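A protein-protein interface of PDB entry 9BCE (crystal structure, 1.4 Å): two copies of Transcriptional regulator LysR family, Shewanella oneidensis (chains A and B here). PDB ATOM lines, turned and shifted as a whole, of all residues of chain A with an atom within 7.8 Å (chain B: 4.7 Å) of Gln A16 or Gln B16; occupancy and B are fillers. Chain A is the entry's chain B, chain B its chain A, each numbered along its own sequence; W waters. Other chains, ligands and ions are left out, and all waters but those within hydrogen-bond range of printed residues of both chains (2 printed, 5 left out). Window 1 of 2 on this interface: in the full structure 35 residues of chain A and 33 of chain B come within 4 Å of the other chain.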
ATOM      1  N   ILE A  10      21.686  -9.279 -35.495  1.00  0.00           N
ATOM      2  CA  ILE A  10      22.252  -7.933 -35.538  1.00  0.00           C
ATOM      3  C   ILE A  10      23.770  -8.034 -35.469  1.00  0.00           C
ATOM      4  O   ILE A  10      24.275  -8.749 -34.598  1.00  0.00           O
ATOM      5  CB  ILE A  10      21.718  -7.053 -34.393  1.00  0.00           C
ATOM      6  CG1 ILE A  10      20.176  -7.073 -34.343  1.00  0.00           C
ATOM      7  CG2 ILE A  10      22.269  -5.625 -34.507  1.00  0.00           C
ATOM      8  CD1 ILE A  10      19.566  -6.137 -33.304  1.00  0.00           C
ATOM      9  N   PRO A  11      24.542  -7.372 -36.324  1.00  0.00           N
ATOM     10  CA  PRO A  11      26.009  -7.510 -36.258  1.00  0.00           C
ATOM     11  C   PRO A  11      26.529  -7.108 -34.889  1.00  0.00           C
ATOM     12  O   PRO A  11      25.965  -6.240 -34.218  1.00  0.00           O
ATOM     13  CB  PRO A  11      26.503  -6.536 -37.334  1.00  0.00           C
ATOM     14  CG  PRO A  11      25.326  -6.462 -38.303  1.00  0.00           C
ATOM     15  CD  PRO A  11      24.108  -6.517 -37.456  1.00  0.00           C
ATOM     16  N   VAL A  12      27.641  -7.742 -34.486  1.00  0.00           N
ATOM     17  CA  VAL A  12      28.259  -7.441 -33.197  1.00  0.00           C
ATOM     18  C   VAL A  12      28.730  -5.992 -33.105  1.00  0.00           C
ATOM     19  O   VAL A  12      28.842  -5.448 -32.005  1.00  0.00           O
ATOM     20  CB  VAL A  12      29.387  -8.456 -32.914  1.00  0.00           C
ATOM     21  CG1 VAL A  12      30.107  -8.148 -31.584  1.00  0.00           C
ATOM     22  CG2 VAL A  12      28.819  -9.848 -32.863  1.00  0.00           C
ATOM     23  N   SER A  13      28.989  -5.340 -34.238  1.00  0.00           N
ATOM     24  CA  SER A  13      29.404  -3.948 -34.210  1.00  0.00           C
ATOM     25  C   SER A  13      28.294  -2.957 -33.825  1.00  0.00           C
ATOM     26  O   SER A  13      28.622  -1.789 -33.587  1.00  0.00           O
ATOM     27  CB  SER A  13      30.053  -3.569 -35.539  1.00  0.00           C
ATOM     28  OG  SER A  13      29.163  -3.834 -36.615  1.00  0.00           O
ATOM     29  N   PHE A  14      27.020  -3.363 -33.746  1.00  0.00           N
ATOM     30  CA  PHE A  14      25.980  -2.448 -33.242  1.00  0.00           C
ATOM     31  C   PHE A  14      26.115  -2.232 -31.724  1.00  0.00           C
ATOM     32  O   PHE A  14      26.473  -3.139 -30.976  1.00  0.00           O
ATOM     33  CB  PHE A  14      24.586  -3.005 -33.542  1.00  0.00           C
ATOM     34  CG  PHE A  14      23.994  -2.484 -34.815  1.00  0.00           C
ATOM     35  CD1 PHE A  14      24.502  -2.895 -36.030  1.00  0.00           C
ATOM     36  CD2 PHE A  14      22.947  -1.576 -34.798  1.00  0.00           C
ATOM     37  CE1 PHE A  14      23.976  -2.425 -37.215  1.00  0.00           C
ATOM     38  CE2 PHE A  14      22.409  -1.090 -35.990  1.00  0.00           C
ATOM     39  CZ  PHE A  14      22.934  -1.515 -37.202  1.00  0.00           C
ATOM     40  N   SER A  15      25.768  -1.025 -31.255  1.00  0.00           N
ATOM     41  CA  SER A  15      25.828  -0.734 -29.824  1.00  0.00           C
ATOM     42  C   SER A  15      24.726  -1.486 -29.103  1.00  0.00           C
ATOM     43  O   SER A  15      23.547  -1.299 -29.421  1.00  0.00           O
ATOM     44  CB  SER A  15      25.632   0.762 -29.596  1.00  0.00           C
ATOM     45  OG  SER A  15      25.276   1.034 -28.245  1.00  0.00           O
ATOM     46  N   GLN A  16      25.096  -2.283 -28.094  1.00  0.00           N
ATOM     47  CA  GLN A  16      24.091  -2.998 -27.305  1.00  0.00           C
ATOM     48  C   GLN A  16      23.245  -2.043 -26.459  1.00  0.00           C
ATOM     49  O   GLN A  16      22.036  -2.263 -26.271  1.00  0.00           O
ATOM     50  CB  GLN A  16      24.759  -4.086 -26.460  1.00  0.00           C
ATOM     51  CG  GLN A  16      25.372  -5.185 -27.327  1.00  0.00           C
ATOM     52  CD  GLN A  16      26.116  -6.221 -26.555  1.00  0.00           C
ATOM     53  OE1 GLN A  16      25.943  -6.357 -25.340  1.00  0.00           O
ATOM     54  NE2 GLN A  16      26.949  -6.987 -27.249  1.00  0.00           N
ATOM     55  N   GLU A  17      23.855  -0.969 -25.952  1.00  0.00           N
ATOM     56  CA  GLU A  17      23.094   0.071 -25.263  1.00  0.00           C
ATOM     57  C   GLU A  17      22.022   0.668 -26.166  1.00  0.00           C
ATOM     58  O   GLU A  17      20.873   0.867 -25.748  1.00  0.00           O
ATOM     59  CB  GLU A  17      24.053   1.172 -24.820  1.00  0.00           C
ATOM     60  CG  GLU A  17      23.394   2.300 -24.069  1.00  0.00           C
ATOM     61  CD  GLU A  17      24.414   3.186 -23.383  1.00  0.00           C
ATOM     62  OE1 GLU A  17      25.613   3.098 -23.736  1.00  0.00           O
ATOM     63  OE2 GLU A  17      24.018   3.953 -22.485  1.00  0.00           O
ATOM     64  N   LEU A  18      22.393   1.000 -27.400  1.00  0.00           N
ATOM     65  CA  LEU A  18      21.451   1.618 -28.327  1.00  0.00           C
ATOM     66  C   LEU A  18      20.319   0.661 -28.674  1.00  0.00           C
ATOM     67  O   LEU A  18      19.135   1.043 -28.655  1.00  0.00           O
ATOM     68  CB  LEU A  18      22.192   2.069 -29.587  1.00  0.00           C
ATOM     69  CG  LEU A  18      21.646   3.292 -30.324  1.00  0.00           C
ATOM     70  CD1 LEU A  18      21.347   4.438 -29.349  1.00  0.00           C
ATOM     71  CD2 LEU A  18      22.636   3.738 -31.395  1.00  0.00           C
ATOM     72  N   ILE A  19      20.661  -0.591 -28.990  1.00  0.00           N
ATOM     73  CA  ILE A  19      19.625  -1.545 -29.366  1.00  0.00           C
ATOM     74  C   ILE A  19      18.706  -1.840 -28.189  1.00  0.00           C
ATOM     75  O   ILE A  19      17.498  -2.012 -28.369  1.00  0.00           O
ATOM     76  CB  ILE A  19      20.240  -2.811 -29.992  1.00  0.00           C
ATOM     77  CG1 ILE A  19      20.919  -2.453 -31.321  1.00  0.00           C
ATOM     78  CG2 ILE A  19      19.179  -3.915 -30.159  1.00  0.00           C
ATOM     79  CD1 ILE A  19      19.924  -1.984 -32.383  1.00  0.00           C
ATOM     80  N   ALA A  20      19.245  -1.849 -26.965  1.00  0.00           N
ATOM     81  CA  ALA A  20      18.421  -2.049 -25.781  1.00  0.00           C
ATOM     82  C   ALA A  20      17.360  -0.958 -25.642  1.00  0.00           C
ATOM     83  O   ALA A  20      16.181  -1.245 -25.395  1.00  0.00           O
ATOM     84  CB  ALA A  20      19.311  -2.064 -24.546  1.00  0.00           C
ATOM     85  N   ASN A  21      17.767   0.309 -25.797  1.00  0.00           N
ATOM     86  CA  ASN A  21      16.830   1.422 -25.704  1.00  0.00           C
ATOM     87  C   ASN A  21      15.759   1.312 -26.777  1.00  0.00           C
ATOM     88  O   ASN A  21      14.582   1.614 -26.534  1.00  0.00           O
ATOM     89  CB  ASN A  21      17.638   2.721 -25.848  1.00  0.00           C
ATOM     90  CG  ASN A  21      16.793   3.975 -25.777  1.00  0.00           C
ATOM     91  OD1 ASN A  21      16.073   4.310 -26.722  1.00  0.00           O
ATOM     92  ND2 ASN A  21      16.879   4.681 -24.662  1.00  0.00           N
ATOM     93  N   LEU A  22      16.156   0.871 -27.971  1.00  0.00           N
ATOM     94  CA  LEU A  22      15.222   0.712 -29.074  1.00  0.00           C
ATOM     95  C   LEU A  22      14.208  -0.394 -28.784  1.00  0.00           C
ATOM     96  O   LEU A  22      13.000  -0.219 -28.993  1.00  0.00           O
ATOM     97  CB  LEU A  22      16.026   0.423 -30.340  1.00  0.00           C
ATOM     98  CG  LEU A  22      15.271   0.487 -31.665  1.00  0.00           C
ATOM     99  CD1 LEU A  22      16.251   0.865 -32.802  1.00  0.00           C
ATOM    100  CD2 LEU A  22      14.630  -0.852 -31.925  1.00  0.00           C
ATOM    101  N   CYS A  23      14.687  -1.553 -28.326  1.00  0.00           N
ATOM    102  CA  CYS A  23      13.779  -2.664 -28.046  1.00  0.00           C
ATOM    103  C   CYS A  23      12.850  -2.354 -26.885  1.00  0.00           C
ATOM    104  O   CYS A  23      11.694  -2.795 -26.887  1.00  0.00           O
ATOM    105  CB  CYS A  23      14.579  -3.935 -27.775  1.00  0.00           C
ATOM    106  SG  CYS A  23      15.344  -4.613 -29.262  1.00  0.00           S
ATOM    107  N   PHE A  39      23.116 -10.757 -31.168  1.00  0.00           N
ATOM    108  CA  PHE A  39      24.246 -10.038 -31.740  1.00  0.00           C
ATOM    109  C   PHE A  39      25.230 -11.078 -32.252  1.00  0.00           C
ATOM    110  O   PHE A  39      25.792 -11.864 -31.469  1.00  0.00           O
ATOM    111  CB  PHE A  39      24.867  -9.110 -30.704  1.00  0.00           C
ATOM    112  CG  PHE A  39      23.944  -8.021 -30.242  1.00  0.00           C
ATOM    113  CD1 PHE A  39      23.112  -8.220 -29.160  1.00  0.00           C
ATOM    114  CD2 PHE A  39      23.924  -6.790 -30.881  1.00  0.00           C
ATOM    115  CE1 PHE A  39      22.244  -7.218 -28.736  1.00  0.00           C
ATOM    116  CE2 PHE A  39      23.064  -5.771 -30.455  1.00  0.00           C
ATOM    117  CZ  PHE A  39      22.226  -5.988 -29.384  1.00  0.00           C
ATOM    118  N   THR A  40      25.423 -11.109 -33.566  1.00  0.00           N
ATOM    119  CA  THR A  40      26.209 -12.151 -34.195  1.00  0.00           C
ATOM    120  C   THR A  40      26.724 -11.633 -35.528  1.00  0.00           C
ATOM    121  O   THR A  40      26.057 -10.829 -36.198  1.00  0.00           O
ATOM    122  CB  THR A  40      25.365 -13.418 -34.379  1.00  0.00           C
ATOM    123  OG1 THR A  40      26.166 -14.422 -35.002  1.00  0.00           O
ATOM    124  CG2 THR A  40      24.098 -13.132 -35.231  1.00  0.00           C
ATOM    125  N   LEU A 104      38.324  -1.935 -37.885  1.00  0.00           N
ATOM    126  CA  LEU A 104      37.066  -2.545 -37.467  1.00  0.00           C
ATOM    127  C   LEU A 104      36.799  -3.699 -38.419  1.00  0.00           C
ATOM    128  O   LEU A 104      36.566  -3.481 -39.615  1.00  0.00           O
ATOM    129  CB  LEU A 104      35.906  -1.547 -37.487  1.00  0.00           C
ATOM    130  CG  LEU A 104      34.541  -2.112 -37.062  1.00  0.00           C
ATOM    131  CD1 LEU A 104      34.511  -2.385 -35.575  1.00  0.00           C
ATOM    132  CD2 LEU A 104      33.380  -1.219 -37.495  1.00  0.00           C
ATOM    133  N   VAL A 132      39.594  -5.356 -34.429  1.00  0.00           N
ATOM    134  CA  VAL A 132      38.573  -5.693 -33.442  1.00  0.00           C
ATOM    135  C   VAL A 132      37.234  -5.468 -34.102  1.00  0.00           C
ATOM    136  O   VAL A 132      37.107  -4.613 -34.971  1.00  0.00           O
ATOM    137  CB  VAL A 132      38.745  -4.860 -32.141  1.00  0.00           C
ATOM    138  CG1 VAL A 132      38.583  -3.354 -32.401  1.00  0.00           C
ATOM    139  CG2 VAL A 132      37.798  -5.355 -31.024  1.00  0.00           C
ATOM    140  N   ASN A 133      36.218  -6.208 -33.665  1.00  0.00           N
ATOM    141  CA  ASN A 133      34.882  -6.072 -34.235  1.00  0.00           C
ATOM    142  C   ASN A 133      33.964  -5.249 -33.339  1.00  0.00           C
ATOM    143  O   ASN A 133      32.749  -5.424 -33.371  1.00  0.00           O
ATOM    144  CB  ASN A 133      34.285  -7.437 -34.616  1.00  0.00           C
ATOM    145  CG  ASN A 133      34.010  -8.322 -33.420  1.00  0.00           C
ATOM    146  OD1 ASN A 133      34.695  -8.209 -32.411  1.00  0.00           O
ATOM    147  ND2 ASN A 133      33.035  -9.238 -33.543  1.00  0.00           N
ATOM    148  N   SER A 134      34.539  -4.316 -32.583  1.00  0.00           N
ATOM    149  CA  SER A 134      33.814  -3.472 -31.629  1.00  0.00           C
ATOM    150  C   SER A 134      34.099  -1.995 -31.889  1.00  0.00           C
ATOM    151  O   SER A 134      35.228  -1.535 -31.619  1.00  0.00           O
ATOM    152  CB  SER A 134      34.275  -3.789 -30.209  1.00  0.00           C
ATOM    153  OG  SER A 134      33.775  -2.799 -29.304  1.00  0.00           O
ATOM    154  N   PRO A 135      33.114  -1.209 -32.334  1.00  0.00           N
ATOM    155  CA  PRO A 135      33.333   0.245 -32.457  1.00  0.00           C
ATOM    156  C   PRO A 135      33.651   0.927 -31.148  1.00  0.00           C
ATOM    157  O   PRO A 135      34.340   1.960 -31.138  1.00  0.00           O
ATOM    158  CB  PRO A 135      32.011   0.745 -33.056  1.00  0.00           C
ATOM    159  CG  PRO A 135      31.502  -0.442 -33.839  1.00  0.00           C
ATOM    160  CD  PRO A 135      31.865  -1.642 -32.991  1.00  0.00           C
ATOM    161  N   ILE A 136      33.148   0.391 -30.035  1.00  0.00           N
ATOM    162  CA  ILE A 136      33.474   0.960 -28.733  1.00  0.00           C
ATOM    163  C   ILE A 136      34.979   0.917 -28.520  1.00  0.00           C
ATOM    164  O   ILE A 136      35.610   1.909 -28.113  1.00  0.00           O
ATOM    165  CB  ILE A 136      32.723   0.193 -27.625  1.00  0.00           C
ATOM    166  CG1 ILE A 136      31.235   0.522 -27.687  1.00  0.00           C
ATOM    167  CG2 ILE A 136      33.297   0.517 -26.244  1.00  0.00           C
ATOM    168  CD1 ILE A 136      30.398  -0.416 -26.855  1.00  0.00           C
ATOM    169  N   MET A 137      35.580  -0.231 -28.815  1.00  0.00           N
ATOM    170  CA  MET A 137      37.019  -0.354 -28.657  1.00  0.00           C
ATOM    171  C   MET A 137      37.814   0.448 -29.693  1.00  0.00           C
ATOM    172  O   MET A 137      38.831   1.053 -29.350  1.00  0.00           O
ATOM    173  CB  MET A 137      37.432  -1.828 -28.576  1.00  0.00           C
ATOM    174  CG  MET A 137      38.904  -2.022 -28.364  1.00  0.00           C
ATOM    175  SD  MET A 137      39.299  -3.831 -27.777  1.00  0.00           S
ATOM    176  CE  MET A 137      41.018  -4.103 -28.638  1.00  0.00           C
ATOM    177  N   VAL A 138      37.341   0.482 -30.946  1.00  0.00           N
ATOM    178  CA  VAL A 138      37.997   1.312 -31.957  1.00  0.00           C
ATOM    179  C   VAL A 138      38.074   2.759 -31.486  1.00  0.00           C
ATOM    180  O   VAL A 138      39.130   3.400 -31.567  1.00  0.00           O
ATOM    181  CB  VAL A 138      37.277   1.196 -33.311  1.00  0.00           C
ATOM    182  CG1 VAL A 138      37.854   2.198 -34.317  1.00  0.00           C
ATOM    183  CG2 VAL A 138      37.380  -0.247 -33.852  1.00  0.00           C
ATOM    184  N   GLN A 140      37.786   4.083 -28.388  1.00  0.00           N
ATOM    185  CA  GLN A 140      38.656   4.278 -27.232  1.00  0.00           C
ATOM    186  C   GLN A 140      40.118   4.249 -27.639  1.00  0.00           C
ATOM    187  O   GLN A 140      40.923   5.061 -27.148  1.00  0.00           O
ATOM    188  CB  GLN A 140      38.394   3.202 -26.172  1.00  0.00           C
ATOM    189  CG  GLN A 140      39.105   3.542 -24.872  1.00  0.00           C
ATOM    190  CD  GLN A 140      38.624   4.880 -24.297  1.00  0.00           C
ATOM    191  OE1 GLN A 140      37.430   5.074 -24.069  1.00  0.00           O
ATOM    192  NE2 GLN A 140      39.553   5.807 -24.078  1.00  0.00           N
ATOM    193  N   VAL B  12      30.259 -12.570 -26.774  1.00  0.00           N
ATOM    194  CA  VAL B  12      29.547 -11.346 -27.152  1.00  0.00           C
ATOM    195  C   VAL B  12      28.909 -10.675 -25.941  1.00  0.00           C
ATOM    196  O   VAL B  12      28.688  -9.452 -25.940  1.00  0.00           O
ATOM    197  CB  VAL B  12      28.546 -11.629 -28.303  1.00  0.00           C
ATOM    198  CG1 VAL B  12      27.701 -10.378 -28.652  1.00  0.00           C
ATOM    199  CG2 VAL B  12      29.318 -12.079 -29.523  1.00  0.00           C
ATOM    200  N   PHE B  14      30.370 -10.174 -23.173  1.00  0.00           N
ATOM    201  CA  PHE B  14      31.393  -9.574 -22.336  1.00  0.00           C
ATOM    202  C   PHE B  14      31.499  -8.081 -22.627  1.00  0.00           C
ATOM    203  O   PHE B  14      31.387  -7.646 -23.774  1.00  0.00           O
ATOM    204  CB  PHE B  14      32.728 -10.288 -22.591  1.00  0.00           C
ATOM    205  CG  PHE B  14      33.670 -10.222 -21.445  1.00  0.00           C
ATOM    206  CD1 PHE B  14      34.545  -9.162 -21.322  1.00  0.00           C
ATOM    207  CD2 PHE B  14      33.652 -11.193 -20.454  1.00  0.00           C
ATOM    208  CE1 PHE B  14      35.419  -9.086 -20.238  1.00  0.00           C
ATOM    209  CE2 PHE B  14      34.510 -11.129 -19.381  1.00  0.00           C
ATOM    210  CZ  PHE B  14      35.396 -10.074 -19.273  1.00  0.00           C
ATOM    211  N   SER B  15      31.727  -7.293 -21.584  1.00  0.00           N
ATOM    212  CA  SER B  15      31.773  -5.840 -21.711  1.00  0.00           C
ATOM    213  C   SER B  15      32.847  -5.368 -22.697  1.00  0.00           C
ATOM    214  O   SER B  15      34.048  -5.548 -22.455  1.00  0.00           O
ATOM    215  CB  SER B  15      32.054  -5.236 -20.339  1.00  0.00           C
ATOM    216  OG  SER B  15      32.289  -3.839 -20.454  1.00  0.00           O
ATOM    217  N   GLN B  16      32.413  -4.705 -23.780  1.00  0.00           N
ATOM    218  CA  GLN B  16      33.372  -4.162 -24.737  1.00  0.00           C
ATOM    219  C   GLN B  16      34.146  -2.996 -24.135  1.00  0.00           C
ATOM    220  O   GLN B  16      35.333  -2.819 -24.426  1.00  0.00           O
ATOM    221  CB  GLN B  16      32.659  -3.749 -26.033  1.00  0.00           C
ATOM    222  CG  GLN B  16      32.240  -4.953 -26.857  1.00  0.00           C
ATOM    223  CD  GLN B  16      31.229  -4.623 -27.950  1.00  0.00           C
ATOM    224  OE1 GLN B  16      31.369  -3.643 -28.691  1.00  0.00           O
ATOM    225  NE2 GLN B  16      30.205  -5.459 -28.051  1.00  0.00           N
ATOM    226  N   GLU B  17      33.485  -2.198 -23.298  1.00  0.00           N
ATOM    227  CA  GLU B  17      34.145  -1.097 -22.604  1.00  0.00           C
ATOM    228  C   GLU B  17      35.260  -1.587 -21.690  1.00  0.00           C
ATOM    229  O   GLU B  17      36.356  -1.011 -21.679  1.00  0.00           O
ATOM    230  CB  GLU B  17      33.097  -0.295 -21.834  1.00  0.00           C
ATOM    231  CG  GLU B  17      33.624   0.943 -21.146  1.00  0.00           C
ATOM    232  CD  GLU B  17      32.535   1.731 -20.417  1.00  0.00           C
ATOM    233  OE1 GLU B  17      31.337   1.457 -20.654  1.00  0.00           O
ATOM    234  OE2 GLU B  17      32.881   2.594 -19.583  1.00  0.00           O
ATOM    235  N   LEU B  18      35.020  -2.673 -20.947  1.00  0.00           N
ATOM    236  CA  LEU B  18      36.057  -3.217 -20.069  1.00  0.00           C
ATOM    237  C   LEU B  18      37.255  -3.707 -20.880  1.00  0.00           C
ATOM    238  O   LEU B  18      38.416  -3.420 -20.545  1.00  0.00           O
ATOM    239  CB  LEU B  18      35.471  -4.371 -19.244  1.00  0.00           C
ATOM    240  CG  LEU B  18      36.432  -5.184 -18.370  1.00  0.00           C
ATOM    241  CD1 LEU B  18      37.194  -4.287 -17.408  1.00  0.00           C
ATOM    242  CD2 LEU B  18      35.656  -6.277 -17.620  1.00  0.00           C
ATOM    243  N   ILE B  19      36.989  -4.460 -21.948  1.00  0.00           N
ATOM    244  CA  ILE B  19      38.067  -4.984 -22.780  1.00  0.00           C
ATOM    245  C   ILE B  19      38.845  -3.846 -23.429  1.00  0.00           C
ATOM    246  O   ILE B  19      40.074  -3.895 -23.529  1.00  0.00           O
ATOM    247  CB  ILE B  19      37.506  -5.988 -23.807  1.00  0.00           C
ATOM    248  CG1 ILE B  19      36.980  -7.239 -23.087  1.00  0.00           C
ATOM    249  CG2 ILE B  19      38.565  -6.381 -24.840  1.00  0.00           C
ATOM    250  CD1 ILE B  19      38.007  -8.016 -22.249  1.00  0.00           C
ATOM    251  N   ALA B  20      38.146  -2.800 -23.880  1.00  0.00           N
ATOM    252  CA  ALA B  20      38.848  -1.676 -24.496  1.00  0.00           C
ATOM    253  C   ALA B  20      39.830  -1.037 -23.525  1.00  0.00           C
ATOM    254  O   ALA B  20      40.970  -0.719 -23.900  1.00  0.00           O
ATOM    255  CB  ALA B  20      37.847  -0.650 -25.019  1.00  0.00           C
ATOM    256  N   PHE B  39      34.907 -10.450 -30.591  1.00  0.00           N
ATOM    257  CA  PHE B  39      33.758 -10.790 -29.762  1.00  0.00           C
ATOM    258  C   PHE B  39      32.903 -11.755 -30.568  1.00  0.00           C
ATOM    259  O   PHE B  39      32.377 -11.392 -31.633  1.00  0.00           O
ATOM    260  CB  PHE B  39      32.980  -9.528 -29.376  1.00  0.00           C
ATOM    261  CG  PHE B  39      33.766  -8.600 -28.471  1.00  0.00           C
ATOM    262  CD1 PHE B  39      34.645  -7.672 -29.001  1.00  0.00           C
ATOM    263  CD2 PHE B  39      33.686  -8.722 -27.080  1.00  0.00           C
ATOM    264  CE1 PHE B  39      35.418  -6.848 -28.167  1.00  0.00           C
ATOM    265  CE2 PHE B  39      34.445  -7.894 -26.245  1.00  0.00           C
ATOM    266  CZ  PHE B  39      35.317  -6.957 -26.790  1.00  0.00           C
ATOM    267  N   SER B 134      23.144 -10.248 -24.514  1.00  0.00           N
ATOM    268  CA  SER B 134      23.700  -8.974 -24.051  1.00  0.00           C
ATOM    269  C   SER B 134      23.269  -8.639 -22.622  1.00  0.00           C
ATOM    270  O   SER B 134      22.095  -8.329 -22.401  1.00  0.00           O
ATOM    271  CB  SER B 134      23.188  -7.845 -24.952  1.00  0.00           C
ATOM    272  OG  SER B 134      23.480  -6.573 -24.396  1.00  0.00           O
ATOM    273  N   PRO B 135      24.186  -8.659 -21.644  1.00  0.00           N
ATOM    274  CA  PRO B 135      23.838  -8.211 -20.282  1.00  0.00           C
ATOM    275  C   PRO B 135      23.408  -6.758 -20.211  1.00  0.00           C
ATOM    276  O   PRO B 135      22.642  -6.387 -19.304  1.00  0.00           O
ATOM    277  CB  PRO B 135      25.140  -8.454 -19.491  1.00  0.00           C
ATOM    278  CG  PRO B 135      25.858  -9.510 -20.247  1.00  0.00           C
ATOM    279  CD  PRO B 135      25.538  -9.235 -21.707  1.00  0.00           C
ATOM    280  N   ILE B 136      23.880  -5.929 -21.141  1.00  0.00           N
ATOM    281  CA  ILE B 136      23.473  -4.529 -21.179  1.00  0.00           C
ATOM    282  C   ILE B 136      21.986  -4.432 -21.478  1.00  0.00           C
ATOM    283  O   ILE B 136      21.241  -3.723 -20.788  1.00  0.00           O
ATOM    284  CB  ILE B 136      24.324  -3.764 -22.208  1.00  0.00           C
ATOM    285  CG1 ILE B 136      25.754  -3.612 -21.685  1.00  0.00           C
ATOM    286  CG2 ILE B 136      23.723  -2.407 -22.517  1.00  0.00           C
ATOM    287  CD1 ILE B 136      26.732  -3.228 -22.763  1.00  0.00           C
ATOM    288  N   MET B 137      21.524  -5.156 -22.505  1.00  0.00           N
ATOM    289  CA  MET B 137      20.095  -5.145 -22.865  1.00  0.00           C
ATOM    290  C   MET B 137      19.261  -5.807 -21.762  1.00  0.00           C
ATOM    291  O   MET B 137      18.192  -5.319 -21.434  1.00  0.00           O
ATOM    292  CB  MET B 137      19.832  -5.797 -24.254  1.00  0.00           C
ATOM    293  CG  MET B 137      18.333  -5.949 -24.703  1.00  0.00           C
ATOM    294  SD  MET B 137      18.065  -6.060 -26.694  1.00  0.00           S
ATOM    295  CE  MET B 137      19.803  -5.346 -27.111  1.00  0.00           C
HETATM  296  O   HOH W   1      31.877 -12.339 -34.151  1.00  0.00           O
HETATM  297  O   HOH W   2      27.452  -5.692 -29.798  1.00  0.00           O
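The side-chain hydroxyl (OG) of Ser A134 sits at hydrogen-bond distance from the side-chain amide oxygen (OE1) of Gln B16, 2.6 Å away.
The side-chain amide oxygen (OE1) of Gln A16 sits at hydrogen-bond distance from the side-chain hydroxyl (OG) of Ser B134 (2.6 Å).
OD1 of Asn A133 is in hydrogen-bond range of N of Phe B39 (2.9 Å).
O of Val B12 lies within hydrogen-bond range of NE2 of Gln A16.
The backbone NH of Ile B136 sits close to the side-chain hydroxyl of Ser B134 (3.3 Å).
The side-chain hydroxyl of Ser A15 lies close to the backbone NH of Glu A17 (3.4 Å).
The backbone carbonyl oxygen (O) of Ile A19 sits at hydrogen-bond distance from the side-chain sulfur (SG) of Cys A23, at 3.5 Å.
OG of Ser B134 lies within hydrogen-bond range of N of Met B137 (3.1 Å).
OG of Ser A134 sits close to N of Ile A136 (3.3 Å).
The side-chain hydroxyl (OG) of Ser A134 lies within hydrogen-bond range of the backbone NH (N) of Met A137 (3.2 Å).
Among the printed residues, pairs that only touch across the chains: Val A12 with Phe B39 (3.9 Å), Gln A16 with Gln B16 (3.7 Å), Gln A16 with Ile B136 (3.99 Å), Gln A16 with Met B137 (3.9 Å), Glu A17 with Ile B136 (3.7 Å), Ile A19 with Met B137 (3.4 Å), Ala A20 with Met B137 (3.5 Å), Phe A39 with Val B12 (3.7 Å), Phe A39 with Ser B134 (3.95 Å), Phe A39 with Met B137 (3.4 Å), Ser A134 with Phe B39 (3.9 Å), Ile A136 with Gln B16 (3.8 Å), Met A137 with Ile B19 (3.96 Å) and Met A137 with Ala B20 (3.7 Å).
Pro A11 touches none of the printed residues of chain B.
Of the printed residues of chain B, Gln A16 touches Val B12 (3.3 Å), Gln B16 (3.7 Å), Ser B134 (2.6 Å), Ile B136 (3.99 Å) and Met B137 (3.9 Å).
Printed residues of chain B within 4 Å of Ile A19: Met B137.
Printed residues of chain B within 4 Å of Asn A133: Phe B39.
Of the printed residues of chain B, Met A137 touches Ile B19 and Ala B20.
Ser B15 touches none of the printed residues of chain A.
Gln B16 touches just these residues of chain A: Gln A16, Ser A134 and Ile A136.
Printed residues of chain A within 4 Å of Phe B39: Val A12, Asn A133 and Ser A134.
Printed residues of chain A within 4 Å of Ser B134: Gln A16 (2.6 Å) and Phe A39 (3.95 Å).
Pro B135 touches none of the printed residues of chain A.
The nearest printed residue of chain A that does not touch Ser B134 is Glu A17 (5.8 Å).
Of the 13 printed residues of chain B, 8 touch a printed residue of chain A.
Printed residues of chain B that touch a printed residue of chain A: Val B12, Gln B16, Ile B19, Ala B20, Phe B39, Ser B134, Ile B136 and Met B137.
Hydrophobic or aromatic side chains of chain B that line the printed part of chain A: Val B12, Ile B19, Ala B20, Phe B39, Ile B136 and Met B137.
Among the printed residues, no Asp or Glu carboxylate lies within 4 Å of a Lys or Arg side-chain nitrogen of the other chain.
Gln A16 touches Ile B136, and with the chains exchanged Ile A136 touches Gln B16.
Gln A16 touches Met B137, but with the chains exchanged Met A137 does not touch Gln B16 (4.8 Å).
Ile A19 touches Met B137, and with the chains exchanged Met A137 touches Ile B19.
Phe A39 touches Ser B134, and with the chains exchanged Ser A134 touches Phe B39.
Positions printed for both chains: 12, 14, 15, 16, 17, 18, 19, 20, 39, 134, 135, 136 and 137.
Of the 18 pairs that touch across the chains among the printed residues, 13 have their exchanged pair printed and touching as well.
Water W2 lies within hydrogen-bond range of the backbone carbonyl oxygen (O) of Val A12 (2.6 Å), the side-chain amide nitrogen (NE2) of Gln A16 (2.9 Å), the backbone carbonyl oxygen (O) of Phe A14 (3.0 Å) and the side-chain amide nitrogen (NE2) of Gln B16 (3.3 Å).
Water W1 bridges the backbone carbonyl oxygen (O) of Phe B39 (2.7 Å) and the side-chain amide nitrogen (ND2) of Asn A133 (3.4 Å).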
